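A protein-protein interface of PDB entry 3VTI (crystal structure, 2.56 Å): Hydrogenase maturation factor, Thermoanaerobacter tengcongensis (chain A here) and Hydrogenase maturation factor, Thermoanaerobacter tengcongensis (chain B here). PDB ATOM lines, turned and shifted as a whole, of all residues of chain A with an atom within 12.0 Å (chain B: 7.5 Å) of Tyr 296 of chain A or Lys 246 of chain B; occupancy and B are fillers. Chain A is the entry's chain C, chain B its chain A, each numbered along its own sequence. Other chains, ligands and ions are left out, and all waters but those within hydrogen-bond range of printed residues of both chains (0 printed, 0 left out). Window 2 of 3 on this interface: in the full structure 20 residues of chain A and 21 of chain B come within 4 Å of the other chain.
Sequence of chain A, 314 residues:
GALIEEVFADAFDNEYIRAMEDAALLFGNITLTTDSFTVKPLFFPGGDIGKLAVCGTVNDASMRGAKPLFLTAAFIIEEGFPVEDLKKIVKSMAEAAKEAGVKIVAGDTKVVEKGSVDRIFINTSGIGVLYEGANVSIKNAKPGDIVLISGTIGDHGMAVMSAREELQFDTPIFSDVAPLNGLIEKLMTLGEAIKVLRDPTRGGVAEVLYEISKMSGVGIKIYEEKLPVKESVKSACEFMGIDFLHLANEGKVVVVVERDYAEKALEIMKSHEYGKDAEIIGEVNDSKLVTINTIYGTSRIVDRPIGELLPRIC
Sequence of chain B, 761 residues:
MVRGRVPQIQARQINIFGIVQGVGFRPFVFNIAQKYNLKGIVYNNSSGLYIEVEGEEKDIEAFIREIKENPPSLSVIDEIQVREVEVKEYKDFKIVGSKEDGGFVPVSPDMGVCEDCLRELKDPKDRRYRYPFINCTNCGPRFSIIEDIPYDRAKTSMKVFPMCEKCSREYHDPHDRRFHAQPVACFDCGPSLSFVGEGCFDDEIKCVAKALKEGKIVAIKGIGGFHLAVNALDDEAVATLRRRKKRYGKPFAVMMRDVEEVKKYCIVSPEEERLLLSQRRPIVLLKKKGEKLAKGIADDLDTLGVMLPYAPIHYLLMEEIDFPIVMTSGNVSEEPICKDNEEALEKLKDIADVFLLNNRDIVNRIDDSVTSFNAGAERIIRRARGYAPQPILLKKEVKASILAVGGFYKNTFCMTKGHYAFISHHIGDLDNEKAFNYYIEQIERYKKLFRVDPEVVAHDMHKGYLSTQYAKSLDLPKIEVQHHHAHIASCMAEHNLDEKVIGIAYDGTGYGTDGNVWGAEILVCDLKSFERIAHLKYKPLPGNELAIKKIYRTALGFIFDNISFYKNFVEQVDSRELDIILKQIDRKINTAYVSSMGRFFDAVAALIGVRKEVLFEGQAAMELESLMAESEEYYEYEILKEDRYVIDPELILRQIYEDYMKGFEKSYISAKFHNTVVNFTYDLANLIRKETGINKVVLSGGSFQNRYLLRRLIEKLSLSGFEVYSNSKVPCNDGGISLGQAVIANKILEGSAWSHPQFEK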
ATOM      1  N   LYS A 221     -20.277  23.561   1.053  1.00  0.00           N
ATOM      2  CA  LYS A 221     -20.838  22.432   1.718  1.00  0.00           C
ATOM      3  C   LYS A 221     -20.196  21.158   1.262  1.00  0.00           C
ATOM      4  O   LYS A 221     -20.175  20.850   0.103  1.00  0.00           O
ATOM      5  CB  LYS A 221     -22.330  22.372   1.479  1.00  0.00           C
ATOM      6  CG  LYS A 221     -23.012  21.269   2.227  1.00  0.00           C
ATOM      7  CD  LYS A 221     -24.476  21.550   2.373  1.00  0.00           C
ATOM      8  CE  LYS A 221     -24.763  22.488   3.513  1.00  0.00           C
ATOM      9  NZ  LYS A 221     -25.506  21.826   4.592  1.00  0.00           N
ATOM     10  N   ILE A 222     -19.668  20.418   2.210  1.00  0.00           N
ATOM     11  CA  ILE A 222     -19.120  19.095   1.927  1.00  0.00           C
ATOM     12  C   ILE A 222     -19.910  17.951   2.585  1.00  0.00           C
ATOM     13  O   ILE A 222     -20.729  18.162   3.489  1.00  0.00           O
ATOM     14  CB  ILE A 222     -17.606  18.994   2.241  1.00  0.00           C
ATOM     15  CG1 ILE A 222     -17.333  19.195   3.735  1.00  0.00           C
ATOM     16  CG2 ILE A 222     -16.822  19.982   1.381  1.00  0.00           C
ATOM     17  CD1 ILE A 222     -15.876  18.968   4.148  1.00  0.00           C
ATOM     18  N   TYR A 223     -19.657  16.735   2.108  1.00  0.00           N
ATOM     19  CA  TYR A 223     -20.419  15.563   2.528  1.00  0.00           C
ATOM     20  C   TYR A 223     -19.518  14.520   3.172  1.00  0.00           C
ATOM     21  O   TYR A 223     -18.593  14.003   2.543  1.00  0.00           O
ATOM     22  CB  TYR A 223     -21.239  14.998   1.353  1.00  0.00           C
ATOM     23  CG  TYR A 223     -22.290  15.982   0.876  1.00  0.00           C
ATOM     24  CD1 TYR A 223     -23.583  15.958   1.397  1.00  0.00           C
ATOM     25  CD2 TYR A 223     -21.975  16.974  -0.058  1.00  0.00           C
ATOM     26  CE1 TYR A 223     -24.548  16.886   0.980  1.00  0.00           C
ATOM     27  CE2 TYR A 223     -22.923  17.903  -0.477  1.00  0.00           C
ATOM     28  CZ  TYR A 223     -24.207  17.853   0.044  1.00  0.00           C
ATOM     29  OH  TYR A 223     -25.144  18.771  -0.367  1.00  0.00           O
ATOM     30  N   GLU A 224     -19.794  14.238   4.442  1.00  0.00           N
ATOM     31  CA  GLU A 224     -19.030  13.272   5.231  1.00  0.00           C
ATOM     32  C   GLU A 224     -18.804  11.937   4.515  1.00  0.00           C
ATOM     33  O   GLU A 224     -17.663  11.499   4.377  1.00  0.00           O
ATOM     34  CB  GLU A 224     -19.719  13.038   6.578  1.00  0.00           C
ATOM     35  CG  GLU A 224     -18.973  12.098   7.513  1.00  0.00           C
ATOM     36  CD  GLU A 224     -19.669  11.958   8.853  1.00  0.00           C
ATOM     37  OE1 GLU A 224     -20.870  11.574   8.877  1.00  0.00           O
ATOM     38  OE2 GLU A 224     -19.010  12.233   9.880  1.00  0.00           O
ATOM     39  N   GLU A 225     -19.893  11.317   4.063  1.00  0.00           N
ATOM     40  CA  GLU A 225     -19.858  10.026   3.365  1.00  0.00           C
ATOM     41  C   GLU A 225     -19.040  10.017   2.072  1.00  0.00           C
ATOM     42  O   GLU A 225     -18.626   8.955   1.608  1.00  0.00           O
ATOM     43  CB  GLU A 225     -21.280   9.531   3.057  1.00  0.00           C
ATOM     44  CG  GLU A 225     -22.222  10.591   2.481  1.00  0.00           C
ATOM     45  CD  GLU A 225     -22.809  11.497   3.566  1.00  0.00           C
ATOM     46  OE1 GLU A 225     -23.483  10.962   4.472  1.00  0.00           O
ATOM     47  OE2 GLU A 225     -22.585  12.733   3.527  1.00  0.00           O
ATOM     48  N   LYS A 226     -18.813  11.198   1.504  1.00  0.00           N
ATOM     49  CA  LYS A 226     -18.104  11.326   0.238  1.00  0.00           C
ATOM     50  C   LYS A 226     -16.623  11.635   0.397  1.00  0.00           C
ATOM     51  O   LYS A 226     -15.907  11.701  -0.595  1.00  0.00           O
ATOM     52  CB  LYS A 226     -18.766  12.394  -0.643  1.00  0.00           C
ATOM     53  CG  LYS A 226     -20.067  11.947  -1.316  1.00  0.00           C
ATOM     54  CD  LYS A 226     -19.807  10.906  -2.407  1.00  0.00           C
ATOM     55  CE  LYS A 226     -21.059  10.100  -2.720  1.00  0.00           C
ATOM     56  NZ  LYS A 226     -21.355   9.101  -1.650  1.00  0.00           N
ATOM     57  N   ILE A 292     -20.476  20.983   6.850  1.00  0.00           N
ATOM     58  CA  ILE A 292     -20.377  19.566   6.497  1.00  0.00           C
ATOM     59  C   ILE A 292     -21.661  18.814   6.855  1.00  0.00           C
ATOM     60  O   ILE A 292     -22.169  18.919   7.971  1.00  0.00           O
ATOM     61  CB  ILE A 292     -19.137  18.884   7.146  1.00  0.00           C
ATOM     62  CG1 ILE A 292     -19.058  17.407   6.743  1.00  0.00           C
ATOM     63  CG2 ILE A 292     -19.139  19.064   8.663  1.00  0.00           C
ATOM     64  CD1 ILE A 292     -17.806  16.698   7.192  1.00  0.00           C
ATOM     65  N   ASN A 293     -22.179  18.065   5.890  1.00  0.00           N
ATOM     66  CA  ASN A 293     -23.370  17.249   6.092  1.00  0.00           C
ATOM     67  C   ASN A 293     -23.008  15.809   6.406  1.00  0.00           C
ATOM     68  O   ASN A 293     -22.202  15.198   5.701  1.00  0.00           O
ATOM     69  CB  ASN A 293     -24.273  17.289   4.853  1.00  0.00           C
ATOM     70  CG  ASN A 293     -25.363  18.340   4.950  1.00  0.00           C
ATOM     71  OD1 ASN A 293     -25.152  19.432   5.475  1.00  0.00           O
ATOM     72  ND2 ASN A 293     -26.543  18.011   4.435  1.00  0.00           N
ATOM     73  N   THR A 294     -23.604  15.275   7.469  1.00  0.00           N
ATOM     74  CA  THR A 294     -23.463  13.861   7.807  1.00  0.00           C
ATOM     75  C   THR A 294     -24.552  13.059   7.087  1.00  0.00           C
ATOM     76  O   THR A 294     -25.366  13.627   6.341  1.00  0.00           O
ATOM     77  CB  THR A 294     -23.551  13.618   9.336  1.00  0.00           C
ATOM     78  OG1 THR A 294     -24.893  13.845   9.788  1.00  0.00           O
ATOM     79  CG2 THR A 294     -22.593  14.527  10.103  1.00  0.00           C
ATOM     80  N   ILE A 295     -24.553  11.742   7.298  1.00  0.00           N
ATOM     81  CA  ILE A 295     -25.628  10.875   6.807  1.00  0.00           C
ATOM     82  C   ILE A 295     -26.990  11.338   7.348  1.00  0.00           C
ATOM     83  O   ILE A 295     -27.117  11.681   8.536  1.00  0.00           O
ATOM     84  CB  ILE A 295     -25.389   9.356   7.134  1.00  0.00           C
ATOM     85  CG1 ILE A 295     -25.078   9.135   8.628  1.00  0.00           C
ATOM     86  CG2 ILE A 295     -24.275   8.777   6.267  1.00  0.00           C
ATOM     87  CD1 ILE A 295     -25.184   7.674   9.096  1.00  0.00           C
ATOM     88  N   TYR A 296     -27.987  11.360   6.458  1.00  0.00           N
ATOM     89  CA  TYR A 296     -29.379  11.726   6.785  1.00  0.00           C
ATOM     90  C   TYR A 296     -29.702  13.237   6.702  1.00  0.00           C
ATOM     91  O   TYR A 296     -30.875  13.627   6.671  1.00  0.00           O
ATOM     92  CB  TYR A 296     -29.843  11.089   8.114  1.00  0.00           C
ATOM     93  CG  TYR A 296     -29.918   9.569   8.060  1.00  0.00           C
ATOM     94  CD1 TYR A 296     -31.132   8.922   7.777  1.00  0.00           C
ATOM     95  CD2 TYR A 296     -28.774   8.778   8.278  1.00  0.00           C
ATOM     96  CE1 TYR A 296     -31.210   7.527   7.719  1.00  0.00           C
ATOM     97  CE2 TYR A 296     -28.838   7.385   8.214  1.00  0.00           C
ATOM     98  CZ  TYR A 296     -30.060   6.767   7.936  1.00  0.00           C
ATOM     99  OH  TYR A 296     -30.139   5.394   7.876  1.00  0.00           O
ATOM    100  N   GLY A 297     -28.665  14.071   6.659  1.00  0.00           N
ATOM    101  CA  GLY A 297     -28.833  15.513   6.473  1.00  0.00           C
ATOM    102  C   GLY A 297     -28.688  16.345   7.736  1.00  0.00           C
ATOM    103  O   GLY A 297     -29.498  17.240   7.986  1.00  0.00           O
ATOM    104  N   THR A 298     -27.653  16.052   8.524  1.00  0.00           N
ATOM    105  CA  THR A 298     -27.358  16.803   9.742  1.00  0.00           C
ATOM    106  C   THR A 298     -26.180  17.738   9.503  1.00  0.00           C
ATOM    107  O   THR A 298     -25.023  17.319   9.485  1.00  0.00           O
ATOM    108  CB  THR A 298     -27.074  15.869  10.929  1.00  0.00           C
ATOM    109  OG1 THR A 298     -28.199  15.006  11.123  1.00  0.00           O
ATOM    110  CG2 THR A 298     -26.818  16.663  12.210  1.00  0.00           C
ATOM    111  N   SER A 299     -26.495  19.012   9.323  1.00  0.00           N
ATOM    112  CA  SER A 299     -25.502  20.014   8.978  1.00  0.00           C
ATOM    113  C   SER A 299     -24.807  20.586  10.220  1.00  0.00           C
ATOM    114  O   SER A 299     -25.440  20.800  11.256  1.00  0.00           O
ATOM    115  CB  SER A 299     -26.171  21.129   8.173  1.00  0.00           C
ATOM    116  OG  SER A 299     -25.216  21.916   7.493  1.00  0.00           O
ATOM    117  N   ARG A 300     -23.498  20.807  10.110  1.00  0.00           N
ATOM    118  CA  ARG A 300     -22.730  21.524  11.131  1.00  0.00           C
ATOM    119  C   ARG A 300     -21.559  22.271  10.490  1.00  0.00           C
ATOM    120  O   ARG A 300     -21.053  21.863   9.441  1.00  0.00           O
ATOM    121  CB  ARG A 300     -22.242  20.585  12.245  1.00  0.00           C
ATOM    122  CG  ARG A 300     -21.305  19.485  11.776  1.00  0.00           C
ATOM    123  CD  ARG A 300     -20.594  18.805  12.932  1.00  0.00           C
ATOM    124  NE  ARG A 300     -19.476  17.993  12.450  1.00  0.00           N
ATOM    125  CZ  ARG A 300     -18.206  18.398  12.413  1.00  0.00           C
ATOM    126  NH1 ARG A 300     -17.870  19.612  12.846  1.00  0.00           N
ATOM    127  NH2 ARG A 300     -17.265  17.582  11.948  1.00  0.00           N
ATOM    128  N   THR B 240     -39.906   3.993  15.845  1.00  0.00           N
ATOM    129  CA  THR B 240     -39.712   4.418  14.454  1.00  0.00           C
ATOM    130  C   THR B 240     -39.325   5.895  14.361  1.00  0.00           C
ATOM    131  O   THR B 240     -38.603   6.292  13.445  1.00  0.00           O
ATOM    132  CB  THR B 240     -40.943   4.146  13.546  1.00  0.00           C
ATOM    133  OG1 THR B 240     -42.068   4.878  14.037  1.00  0.00           O
ATOM    134  CG2 THR B 240     -41.290   2.663  13.503  1.00  0.00           C
ATOM    135  N   LEU B 241     -39.800   6.699  15.314  1.00  0.00           N
ATOM    136  CA  LEU B 241     -39.395   8.102  15.425  1.00  0.00           C
ATOM    137  C   LEU B 241     -37.942   8.218  15.891  1.00  0.00           C
ATOM    138  O   LEU B 241     -37.207   9.084  15.421  1.00  0.00           O
ATOM    139  CB  LEU B 241     -40.337   8.869  16.363  1.00  0.00           C
ATOM    140  CG  LEU B 241     -40.175  10.385  16.541  1.00  0.00           C
ATOM    141  CD1 LEU B 241     -40.392  11.116  15.235  1.00  0.00           C
ATOM    142  CD2 LEU B 241     -41.137  10.909  17.595  1.00  0.00           C
ATOM    143  N   ARG B 242     -37.541   7.344  16.814  1.00  0.00           N
ATOM    144  CA  ARG B 242     -36.149   7.253  17.282  1.00  0.00           C
ATOM    145  C   ARG B 242     -35.205   6.886  16.143  1.00  0.00           C
ATOM    146  O   ARG B 242     -34.117   7.447  16.029  1.00  0.00           O
ATOM    147  CB  ARG B 242     -36.005   6.210  18.396  1.00  0.00           C
ATOM    148  CG  ARG B 242     -36.467   6.675  19.758  1.00  0.00           C
ATOM    149  CD  ARG B 242     -35.391   7.439  20.514  1.00  0.00           C
ATOM    150  NE  ARG B 242     -35.942   8.037  21.720  1.00  0.00           N
ATOM    151  CZ  ARG B 242     -35.470   9.137  22.292  1.00  0.00           C
ATOM    152  NH1 ARG B 242     -34.428   9.765  21.771  1.00  0.00           N
ATOM    153  NH2 ARG B 242     -36.044   9.617  23.387  1.00  0.00           N
ATOM    154  N   ARG B 243     -35.638   5.933  15.320  1.00  0.00           N
ATOM    155  CA  ARG B 243     -34.892   5.481  14.152  1.00  0.00           C
ATOM    156  C   ARG B 243     -34.817   6.574  13.090  1.00  0.00           C
ATOM    157  O   ARG B 243     -33.771   6.756  12.463  1.00  0.00           O
ATOM    158  CB  ARG B 243     -35.559   4.235  13.561  1.00  0.00           C
ATOM    159  CG  ARG B 243     -34.683   3.400  12.616  1.00  0.00           C
ATOM    160  CD  ARG B 243     -35.490   2.298  11.901  1.00  0.00           C
ATOM    161  NE  ARG B 243     -36.424   1.628  12.808  1.00  0.00           N
ATOM    162  CZ  ARG B 243     -37.750   1.700  12.729  1.00  0.00           C
ATOM    163  NH1 ARG B 243     -38.339   2.393  11.754  1.00  0.00           N
ATOM    164  NH2 ARG B 243     -38.491   1.061  13.622  1.00  0.00           N
ATOM    165  N   ARG B 244     -35.923   7.296  12.892  1.00  0.00           N
ATOM    166  CA  ARG B 244     -36.013   8.281  11.809  1.00  0.00           C
ATOM    167  C   ARG B 244     -35.251   9.569  12.110  1.00  0.00           C
ATOM    168  O   ARG B 244     -34.745  10.226  11.195  1.00  0.00           O
ATOM    169  CB  ARG B 244     -37.467   8.552  11.414  1.00  0.00           C
ATOM    170  CG  ARG B 244     -38.067   7.435  10.557  1.00  0.00           C
ATOM    171  CD  ARG B 244     -39.513   7.706  10.182  1.00  0.00           C
ATOM    172  NE  ARG B 244     -40.163   6.547   9.567  1.00  0.00           N
ATOM    173  CZ  ARG B 244     -41.417   6.537   9.127  1.00  0.00           C
ATOM    174  NH1 ARG B 244     -42.170   7.622   9.224  1.00  0.00           N
ATOM    175  NH2 ARG B 244     -41.924   5.443   8.584  1.00  0.00           N
ATOM    176  N   LYS B 245     -35.148   9.916  13.388  1.00  0.00           N
ATOM    177  CA  LYS B 245     -34.304  11.030  13.796  1.00  0.00           C
ATOM    178  C   LYS B 245     -32.865  10.534  13.837  1.00  0.00           C
ATOM    179  O   LYS B 245     -31.958  11.172  13.284  1.00  0.00           O
ATOM    180  CB  LYS B 245     -34.795  11.635  15.110  1.00  0.00           C
ATOM    181  CG  LYS B 245     -36.179  12.309  14.964  1.00  0.00           C
ATOM    182  CD  LYS B 245     -36.346  13.518  15.854  1.00  0.00           C
ATOM    183  CE  LYS B 245     -35.241  14.530  15.609  1.00  0.00           C
ATOM    184  NZ  LYS B 245     -35.485  15.830  16.274  1.00  0.00           N
ATOM    185  N   LYS B 246     -32.678   9.375  14.473  1.00  0.00           N
ATOM    186  CA  LYS B 246     -31.416   8.607  14.465  1.00  0.00           C
ATOM    187  C   LYS B 246     -30.240   9.313  15.140  1.00  0.00           C
ATOM    188  O   LYS B 246     -29.261   8.662  15.509  1.00  0.00           O
ATOM    189  CB  LYS B 246     -31.021   8.159  13.048  1.00  0.00           C
ATOM    190  CG  LYS B 246     -30.222   6.854  13.011  1.00  0.00           C
ATOM    191  CD  LYS B 246     -30.052   6.331  11.581  1.00  0.00           C
ATOM    192  CE  LYS B 246     -29.426   4.925  11.556  1.00  0.00           C
ATOM    193  NZ  LYS B 246     -28.061   4.874  12.172  1.00  0.00           N
ATOM    194  N   ARG B 247     -30.329  10.632  15.298  1.00  0.00           N
ATOM    195  CA  ARG B 247     -29.223  11.404  15.864  1.00  0.00           C
ATOM    196  C   ARG B 247     -29.640  12.093  17.168  1.00  0.00           C
ATOM    197  O   ARG B 247     -28.994  13.053  17.622  1.00  0.00           O
ATOM    198  CB  ARG B 247     -28.710  12.420  14.831  1.00  0.00           C
ATOM    199  CG  ARG B 247     -28.083  11.751  13.600  1.00  0.00           C
ATOM    200  CD  ARG B 247     -27.136  12.660  12.812  1.00  0.00           C
ATOM    201  NE  ARG B 247     -26.380  11.892  11.818  1.00  0.00           N
ATOM    202  CZ  ARG B 247     -25.154  11.398  12.011  1.00  0.00           C
ATOM    203  NH1 ARG B 247     -24.513  11.592  13.159  1.00  0.00           N
ATOM    204  NH2 ARG B 247     -24.560  10.707  11.044  1.00  0.00           N
ATOM    205  N   TYR B 248     -30.718  11.591  17.771  1.00  0.00           N
ATOM    206  CA  TYR B 248     -31.325  12.278  18.902  1.00  0.00           C
ATOM    207  C   TYR B 248     -30.784  11.800  20.261  1.00  0.00           C
ATOM    208  O   TYR B 248     -29.897  12.451  20.832  1.00  0.00           O
ATOM    209  CB  TYR B 248     -32.865  12.255  18.813  1.00  0.00           C
ATOM    210  CG  TYR B 248     -33.519  13.445  19.478  1.00  0.00           C
ATOM    211  CD1 TYR B 248     -33.096  14.743  19.192  1.00  0.00           C
ATOM    212  CD2 TYR B 248     -34.555  13.277  20.390  1.00  0.00           C
ATOM    213  CE1 TYR B 248     -33.682  15.848  19.802  1.00  0.00           C
ATOM    214  CE2 TYR B 248     -35.149  14.383  21.015  1.00  0.00           C
ATOM    215  CZ  TYR B 248     -34.702  15.664  20.713  1.00  0.00           C
ATOM    216  OH  TYR B 248     -35.274  16.763  21.309  1.00  0.00           O
ATOM    217  N   GLY B 249     -31.304  10.679  20.765  1.00  0.00           N
ATOM    218  CA  GLY B 249     -30.953  10.192  22.100  1.00  0.00           C
ATOM    219  C   GLY B 249     -31.712  10.881  23.226  1.00  0.00           C
ATOM    220  O   GLY B 249     -32.087  10.236  24.211  1.00  0.00           O
ATOM    221  N   VAL B 332     -35.165  17.551  11.915  1.00  0.00           N
ATOM    222  CA  VAL B 332     -34.209  16.453  11.894  1.00  0.00           C
ATOM    223  C   VAL B 332     -33.149  16.887  12.897  1.00  0.00           C
ATOM    224  O   VAL B 332     -32.826  18.064  12.968  1.00  0.00           O
ATOM    225  CB  VAL B 332     -33.580  16.201  10.479  1.00  0.00           C
ATOM    226  CG1 VAL B 332     -34.567  16.530   9.353  1.00  0.00           C
ATOM    227  CG2 VAL B 332     -32.296  16.994  10.284  1.00  0.00           C
ATOM    228  N   SER B 333     -32.625  15.966  13.698  1.00  0.00           N
ATOM    229  CA  SER B 333     -31.589  16.320  14.683  1.00  0.00           C
ATOM    230  C   SER B 333     -32.010  17.446  15.663  1.00  0.00           C
ATOM    231  O   SER B 333     -32.979  17.276  16.422  1.00  0.00           O
ATOM    232  CB  SER B 333     -30.267  16.651  13.980  1.00  0.00           C
ATOM    233  OG  SER B 333     -29.178  16.598  14.886  1.00  0.00           O
ATOM    234  N   LYS B 347     -38.125  19.163   4.712  1.00  0.00           N
ATOM    235  CA  LYS B 347     -37.169  18.829   5.765  1.00  0.00           C
ATOM    236  C   LYS B 347     -37.590  17.573   6.540  1.00  0.00           C
ATOM    237  O   LYS B 347     -36.744  16.751   6.914  1.00  0.00           O
ATOM    238  CB  LYS B 347     -37.001  20.020   6.719  1.00  0.00           C
ATOM    239  CG  LYS B 347     -35.714  20.039   7.558  1.00  0.00           C
ATOM    240  CD  LYS B 347     -34.546  20.697   6.794  1.00  0.00           C
ATOM    241  CE  LYS B 347     -33.355  20.980   7.699  1.00  0.00           C
ATOM    242  NZ  LYS B 347     -32.587  19.745   8.012  1.00  0.00           N
ATOM    243  N   LYS B 349     -39.633  15.104   5.464  1.00  0.00           N
ATOM    244  CA  LYS B 349     -40.153  14.085   4.528  1.00  0.00           C
ATOM    245  C   LYS B 349     -39.836  12.645   4.958  1.00  0.00           C
ATOM    246  O   LYS B 349     -40.661  11.745   4.778  1.00  0.00           O
ATOM    247  CB  LYS B 349     -39.648  14.336   3.095  1.00  0.00           C
ATOM    248  CG  LYS B 349     -38.131  14.171   2.931  1.00  0.00           C
ATOM    249  CD  LYS B 349     -37.631  14.602   1.566  1.00  0.00           C
ATOM    250  CE  LYS B 349     -36.120  14.840   1.614  1.00  0.00           C
ATOM    251  NZ  LYS B 349     -35.567  15.169   0.261  1.00  0.00           N
ATOM    252  N   ASP B 350     -38.647  12.443   5.521  1.00  0.00           N
ATOM    253  CA  ASP B 350     -38.197  11.121   5.958  1.00  0.00           C
ATOM    254  C   ASP B 350     -38.554  10.828   7.417  1.00  0.00           C
ATOM    255  O   ASP B 350     -38.191   9.771   7.947  1.00  0.00           O
ATOM    256  CB  ASP B 350     -36.673  10.964   5.781  1.00  0.00           C
ATOM    257  CG  ASP B 350     -36.176  11.382   4.392  1.00  0.00           C
ATOM    258  OD1 ASP B 350     -36.822  11.066   3.357  1.00  0.00           O
ATOM    259  OD2 ASP B 350     -35.107  12.032   4.354  1.00  0.00           O
ATOM    260  N   ILE B 351     -39.240  11.761   8.074  1.00  0.00           N
ATOM    261  CA  ILE B 351     -39.625  11.565   9.469  1.00  0.00           C
ATOM    262  C   ILE B 351     -41.136  11.372   9.587  1.00  0.00           C
ATOM    263  O   ILE B 351     -41.600  10.303   9.978  1.00  0.00           O
ATOM    264  CB  ILE B 351     -39.171  12.738  10.387  1.00  0.00           C
ATOM    265  CG1 ILE B 351     -37.839  13.352   9.924  1.00  0.00           C
ATOM    266  CG2 ILE B 351     -39.140  12.291  11.858  1.00  0.00           C
ATOM    267  CD1 ILE B 351     -36.594  12.812  10.605  1.00  0.00           C
ATOM    268  N   LEU B 615     -25.014   9.597  23.843  1.00  0.00           N
ATOM    269  CA  LEU B 615     -25.636  10.062  22.600  1.00  0.00           C
ATOM    270  C   LEU B 615     -25.737  11.580  22.532  1.00  0.00           C
ATOM    271  O   LEU B 615     -25.865  12.143  21.446  1.00  0.00           O
ATOM    272  CB  LEU B 615     -27.007   9.416  22.403  1.00  0.00           C
ATOM    273  CG  LEU B 615     -26.981   7.883  22.271  1.00  0.00           C
ATOM    274  CD1 LEU B 615     -28.389   7.322  22.422  1.00  0.00           C
ATOM    275  CD2 LEU B 615     -26.348   7.433  20.946  1.00  0.00           C
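The guanidinium group (NE) of Arg 247 of chain B lies within hydrogen-bond range of the side-chain hydroxyl (OG1) of Thr 294 of chain A (3.2 Å). O of Ile 295 of chain A is in hydrogen-bond range of NE of Arg 247 of chain B (3.4 Å).
Among the printed residues, merely in contact across the chains: Tyr 296 of chain A with Lys 246 of chain B, Gly 297 of chain A with Val 332 of chain B, Gly 297 of chain A with Lys 347 of chain B, Thr 298 of chain A with Arg 247 of chain B and Thr 298 of chain A with Ser 333 of chain B.
Printed residues of chain B within 4 Å of Thr 294 of chain A: Arg 247 (3.2 Å). Of chain B, only Lys 246 comes within 4 Å of Tyr 296 of chain A. Printed residues of chain B within 4 Å of Gly 297 of chain A: Val 332 (3.6 Å) and Lys 347 (3.98 Å). No residue of chain A comes within 4 Å of Lys 245 of chain B. Of chain A, only Tyr 296 comes within 4 Å of Lys 246 of chain B. Arg 247 of chain B touches three residues of chain A. No residue of chain A comes within 4 Å of Asp 350 of chain B. The nearest residue of chain B that does not touch Tyr 296 of chain A is Asp 350 of chain B (5.1 Å). The nearest printed residue of chain B that does not touch Gly 297 of chain A is Arg 247 of chain B (6.0 Å).
Of the 15 printed residues of chain A, 5 touch a printed residue of chain B. Printed residues of chain A that touch a printed residue of chain B: Thr 294, Ile 295, Tyr 296, Gly 297 and Thr 298. Of the 17 printed residues of chain B, 5 touch a printed residue of chain A. Printed residues of chain B that touch a printed residue of chain A: Lys 246, Arg 247, Val 332, Ser 333 and Lys 347. Among the printed residues, no Asp or Glu carboxylate lies within 4 Å of a Lys or Arg side-chain nitrogen of the other chain.
The backbone carbonyl oxygen of Ser 333 of chain B is in hydrogen-bond range of the side-chain amino group of Lys 245 of chain B (2.9 Å). The side-chain carboxylate (OE1) of Glu 225 of chain A sits close to the backbone NH (N) of Ile 295 of chain A (3.1 Å). The side-chain hydroxyl (OG1) of Thr 294 of chain A sits close to the backbone carbonyl oxygen (O) of Thr 298 of chain A (3.5 Å).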
